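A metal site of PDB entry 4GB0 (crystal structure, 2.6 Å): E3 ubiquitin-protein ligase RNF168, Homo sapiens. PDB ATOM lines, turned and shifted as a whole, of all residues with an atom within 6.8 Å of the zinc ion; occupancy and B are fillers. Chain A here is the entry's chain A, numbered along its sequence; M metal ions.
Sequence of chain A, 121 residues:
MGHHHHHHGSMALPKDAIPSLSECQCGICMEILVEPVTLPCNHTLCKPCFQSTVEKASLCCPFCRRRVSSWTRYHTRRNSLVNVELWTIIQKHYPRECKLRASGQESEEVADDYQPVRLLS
The zinc ion is bound by the side-chain sulfur (SG) of Cys 46, the side-chain sulfur (SG) of Cys 49, the side-chain sulfur (SG) of Cys 26 and the side-chain sulfur (SG) of Cys 29.
The zinc ion has four donor atoms within binding distance.
The side-chain sulfur (SG) of Cys 46 sits close to the guanidinium group (NH1) of Arg 101 (3.5 Å).
SG of Cys 26 lies close to N of Ile 28 (3.2 Å).
The backbone carbonyl oxygen (O) of Glu 31 sits at hydrogen-bond distance from the backbone NH (N) of Cys 26, at 2.9 Å.
The side-chain sulfur of Cys 29 sits close to the backbone NH of Glu 31, 3.5 Å away.
Along chain A the residues within 4 Å of the zinc ion span positions 26 to 49.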
ATOM      1  N   GLN A  25      -4.719   8.586 -21.628  1.00  0.00           N
ATOM      2  CA  GLN A  25      -5.985   7.979 -21.276  1.00  0.00           C
ATOM      3  C   GLN A  25      -5.933   6.470 -21.496  1.00  0.00           C
ATOM      4  O   GLN A  25      -5.533   6.006 -22.576  1.00  0.00           O
ATOM      5  CB  GLN A  25      -7.123   8.532 -22.140  1.00  0.00           C
ATOM      6  CG  GLN A  25      -7.381  10.028 -22.021  1.00  0.00           C
ATOM      7  CD  GLN A  25      -8.630  10.462 -22.761  1.00  0.00           C
ATOM      8  OE1 GLN A  25      -9.739  10.200 -22.319  1.00  0.00           O
ATOM      9  NE2 GLN A  25      -8.453  11.124 -23.901  1.00  0.00           N
ATOM     10  N   CYS A  26      -6.371   5.712 -20.482  1.00  0.00           N
ATOM     11  CA  CYS A  26      -6.544   4.297 -20.640  1.00  0.00           C
ATOM     12  C   CYS A  26      -7.391   4.045 -21.860  1.00  0.00           C
ATOM     13  O   CYS A  26      -8.435   4.654 -22.029  1.00  0.00           O
ATOM     14  CB  CYS A  26      -7.209   3.703 -19.429  1.00  0.00           C
ATOM     15  SG  CYS A  26      -7.671   2.006 -19.707  1.00  0.00           S
ATOM     16  N   GLY A  27      -6.949   3.130 -22.721  1.00  0.00           N
ATOM     17  CA  GLY A  27      -7.689   2.826 -23.944  1.00  0.00           C
ATOM     18  C   GLY A  27      -8.932   1.968 -23.705  1.00  0.00           C
ATOM     19  O   GLY A  27      -9.737   1.816 -24.623  1.00  0.00           O
ATOM     20  N   ILE A  28      -9.104   1.418 -22.508  1.00  0.00           N
ATOM     21  CA  ILE A  28     -10.292   0.610 -22.230  1.00  0.00           C
ATOM     22  C   ILE A  28     -11.448   1.387 -21.590  1.00  0.00           C
ATOM     23  O   ILE A  28     -12.586   1.193 -21.972  1.00  0.00           O
ATOM     24  CB  ILE A  28      -9.993  -0.657 -21.347  1.00  0.00           C
ATOM     25  CG1 ILE A  28      -9.263  -1.710 -22.138  1.00  0.00           C
ATOM     26  CG2 ILE A  28     -11.248  -1.283 -20.799  1.00  0.00           C
ATOM     27  CD1 ILE A  28      -7.844  -1.793 -21.719  1.00  0.00           C
ATOM     28  N   CYS A  29     -11.165   2.223 -20.598  1.00  0.00           N
ATOM     29  CA  CYS A  29     -12.210   2.895 -19.846  1.00  0.00           C
ATOM     30  C   CYS A  29     -12.295   4.388 -20.169  1.00  0.00           C
ATOM     31  O   CYS A  29     -13.235   5.057 -19.774  1.00  0.00           O
ATOM     32  CB  CYS A  29     -11.980   2.719 -18.347  1.00  0.00           C
ATOM     33  SG  CYS A  29     -10.488   3.555 -17.764  1.00  0.00           S
ATOM     34  N   MET A  30     -11.297   4.911 -20.878  1.00  0.00           N
ATOM     35  CA  MET A  30     -11.278   6.332 -21.252  1.00  0.00           C
ATOM     36  C   MET A  30     -10.914   7.311 -20.120  1.00  0.00           C
ATOM     37  O   MET A  30     -10.700   8.492 -20.388  1.00  0.00           O
ATOM     38  CB  MET A  30     -12.584   6.750 -21.935  1.00  0.00           C
ATOM     39  CG  MET A  30     -12.748   6.189 -23.337  1.00  0.00           C
ATOM     40  SD  MET A  30     -11.213   6.351 -24.293  1.00  0.00           S
ATOM     41  CE  MET A  30     -11.641   5.391 -25.755  1.00  0.00           C
ATOM     42  N   GLU A  31     -10.815   6.830 -18.892  1.00  0.00           N
ATOM     43  CA  GLU A  31     -10.292   7.638 -17.799  1.00  0.00           C
ATOM     44  C   GLU A  31      -8.793   7.934 -17.978  1.00  0.00           C
ATOM     45  O   GLU A  31      -8.148   7.387 -18.864  1.00  0.00           O
ATOM     46  CB  GLU A  31     -10.543   6.953 -16.449  1.00  0.00           C
ATOM     47  CG  GLU A  31     -12.058   6.763 -16.098  1.00  0.00           C
ATOM     48  CD  GLU A  31     -12.882   8.044 -16.363  1.00  0.00           C
ATOM     49  OE1 GLU A  31     -12.616   9.092 -15.722  1.00  0.00           O
ATOM     50  OE2 GLU A  31     -13.782   7.999 -17.234  1.00  0.00           O
ATOM     51  N   ILE A  32      -8.237   8.823 -17.166  1.00  0.00           N
ATOM     52  CA  ILE A  32      -6.807   9.104 -17.143  1.00  0.00           C
ATOM     53  C   ILE A  32      -6.080   7.826 -16.676  1.00  0.00           C
ATOM     54  O   ILE A  32      -6.627   7.063 -15.877  1.00  0.00           O
ATOM     55  CB  ILE A  32      -6.495  10.298 -16.179  1.00  0.00           C
ATOM     56  CG1 ILE A  32      -5.030  10.715 -16.242  1.00  0.00           C
ATOM     57  CG2 ILE A  32      -6.910   9.984 -14.739  1.00  0.00           C
ATOM     58  CD1 ILE A  32      -4.668  11.486 -17.487  1.00  0.00           C
ATOM     59  N   LEU A  33      -4.869   7.592 -17.155  1.00  0.00           N
ATOM     60  CA  LEU A  33      -4.144   6.384 -16.778  1.00  0.00           C
ATOM     61  C   LEU A  33      -3.659   6.471 -15.368  1.00  0.00           C
ATOM     62  O   LEU A  33      -2.691   7.167 -15.066  1.00  0.00           O
ATOM     63  CB  LEU A  33      -2.937   6.129 -17.692  1.00  0.00           C
ATOM     64  CG  LEU A  33      -3.180   5.390 -19.017  1.00  0.00           C
ATOM     65  CD1 LEU A  33      -1.996   5.618 -19.965  1.00  0.00           C
ATOM     66  CD2 LEU A  33      -3.471   3.887 -18.762  1.00  0.00           C
ATOM     67  N   VAL A  34      -4.315   5.725 -14.498  1.00  0.00           N
ATOM     68  CA  VAL A  34      -3.847   5.635 -13.138  1.00  0.00           C
ATOM     69  C   VAL A  34      -3.046   4.352 -12.986  1.00  0.00           C
ATOM     70  O   VAL A  34      -3.527   3.271 -13.342  1.00  0.00           O
ATOM     71  CB  VAL A  34      -5.046   5.685 -12.148  1.00  0.00           C
ATOM     72  CG1 VAL A  34      -4.677   5.128 -10.787  1.00  0.00           C
ATOM     73  CG2 VAL A  34      -5.489   7.127 -11.985  1.00  0.00           C
ATOM     74  N   LEU A  45      -2.652  -0.223 -20.051  1.00  0.00           N
ATOM     75  CA  LEU A  45      -3.989   0.011 -19.544  1.00  0.00           C
ATOM     76  C   LEU A  45      -3.862   0.295 -18.048  1.00  0.00           C
ATOM     77  O   LEU A  45      -2.829  -0.020 -17.448  1.00  0.00           O
ATOM     78  CB  LEU A  45      -4.905  -1.177 -19.834  1.00  0.00           C
ATOM     79  CG  LEU A  45      -4.802  -2.466 -19.013  1.00  0.00           C
ATOM     80  CD1 LEU A  45      -5.820  -3.481 -19.541  1.00  0.00           C
ATOM     81  CD2 LEU A  45      -3.426  -3.040 -19.090  1.00  0.00           C
ATOM     82  N   CYS A  46      -4.885   0.902 -17.460  1.00  0.00           N
ATOM     83  CA  CYS A  46      -4.782   1.329 -16.072  1.00  0.00           C
ATOM     84  C   CYS A  46      -4.920   0.125 -15.166  1.00  0.00           C
ATOM     85  O   CYS A  46      -5.533  -0.858 -15.542  1.00  0.00           O
ATOM     86  CB  CYS A  46      -5.809   2.416 -15.728  1.00  0.00           C
ATOM     87  SG  CYS A  46      -7.519   1.856 -15.420  1.00  0.00           S
ATOM     88  N   LYS A  47      -4.328   0.207 -13.995  1.00  0.00           N
ATOM     89  CA  LYS A  47      -4.385  -0.886 -13.054  1.00  0.00           C
ATOM     90  C   LYS A  47      -5.815  -1.367 -12.803  1.00  0.00           C
ATOM     91  O   LYS A  47      -6.054  -2.563 -12.875  1.00  0.00           O
ATOM     92  CB  LYS A  47      -3.673  -0.520 -11.753  1.00  0.00           C
ATOM     93  CG  LYS A  47      -3.338  -1.725 -10.909  1.00  0.00           C
ATOM     94  CD  LYS A  47      -2.391  -1.338  -9.783  1.00  0.00           C
ATOM     95  CE  LYS A  47      -1.723  -2.568  -9.146  1.00  0.00           C
ATOM     96  NZ  LYS A  47      -0.719  -2.166  -8.099  1.00  0.00           N
ATOM     97  N   PRO A  48      -6.763  -0.449 -12.515  1.00  0.00           N
ATOM     98  CA  PRO A  48      -8.141  -0.921 -12.311  1.00  0.00           C
ATOM     99  C   PRO A  48      -8.628  -1.782 -13.461  1.00  0.00           C
ATOM    100  O   PRO A  48      -9.154  -2.868 -13.212  1.00  0.00           O
ATOM    101  CB  PRO A  48      -8.959   0.377 -12.271  1.00  0.00           C
ATOM    102  CG  PRO A  48      -7.986   1.387 -11.720  1.00  0.00           C
ATOM    103  CD  PRO A  48      -6.641   1.006 -12.299  1.00  0.00           C
ATOM    104  N   CYS A  49      -8.456  -1.299 -14.686  1.00  0.00           N
ATOM    105  CA  CYS A  49      -8.807  -2.106 -15.844  1.00  0.00           C
ATOM    106  C   CYS A  49      -7.999  -3.422 -15.864  1.00  0.00           C
ATOM    107  O   CYS A  49      -8.563  -4.490 -16.072  1.00  0.00           O
ATOM    108  CB  CYS A  49      -8.651  -1.294 -17.133  1.00  0.00           C
ATOM    109  SG  CYS A  49     -10.035  -0.061 -17.428  1.00  0.00           S
ATOM    110  N   PHE A  50      -6.708  -3.364 -15.573  1.00  0.00           N
ATOM    111  CA  PHE A  50      -5.913  -4.562 -15.549  1.00  0.00           C
ATOM    112  C   PHE A  50      -6.540  -5.590 -14.608  1.00  0.00           C
ATOM    113  O   PHE A  50      -6.828  -6.720 -15.004  1.00  0.00           O
ATOM    114  CB  PHE A  50      -4.461  -4.264 -15.196  1.00  0.00           C
ATOM    115  CG  PHE A  50      -3.601  -5.492 -15.038  1.00  0.00           C
ATOM    116  CD1 PHE A  50      -3.197  -6.220 -16.152  1.00  0.00           C
ATOM    117  CD2 PHE A  50      -3.233  -5.934 -13.777  1.00  0.00           C
ATOM    118  CE1 PHE A  50      -2.426  -7.372 -16.012  1.00  0.00           C
ATOM    119  CE2 PHE A  50      -2.460  -7.089 -13.627  1.00  0.00           C
ATOM    120  CZ  PHE A  50      -2.057  -7.800 -14.748  1.00  0.00           C
ATOM    121  N   ARG A 101      -9.362  11.143 -10.121  1.00  0.00           N
ATOM    122  CA  ARG A 101      -9.657   9.712 -10.213  1.00  0.00           C
ATOM    123  C   ARG A 101      -9.467   9.021  -8.883  1.00  0.00           C
ATOM    124  O   ARG A 101     -10.267   8.178  -8.509  1.00  0.00           O
ATOM    125  CB  ARG A 101      -8.834   9.015 -11.289  1.00  0.00           C
ATOM    126  CG  ARG A 101      -9.640   8.679 -12.521  1.00  0.00           C
ATOM    127  CD  ARG A 101      -8.959   7.590 -13.317  1.00  0.00           C
ATOM    128  NE  ARG A 101      -9.421   6.248 -12.969  1.00  0.00           N
ATOM    129  CZ  ARG A 101      -9.069   5.138 -13.624  1.00  0.00           C
ATOM    130  NH1 ARG A 101      -8.240   5.201 -14.675  1.00  0.00           N
ATOM    131  NH2 ARG A 101      -9.538   3.954 -13.223  1.00  0.00           N
HETATM  132 ZN    ZN M   1      -8.617   1.851 -17.458  1.00  0.00          ZN
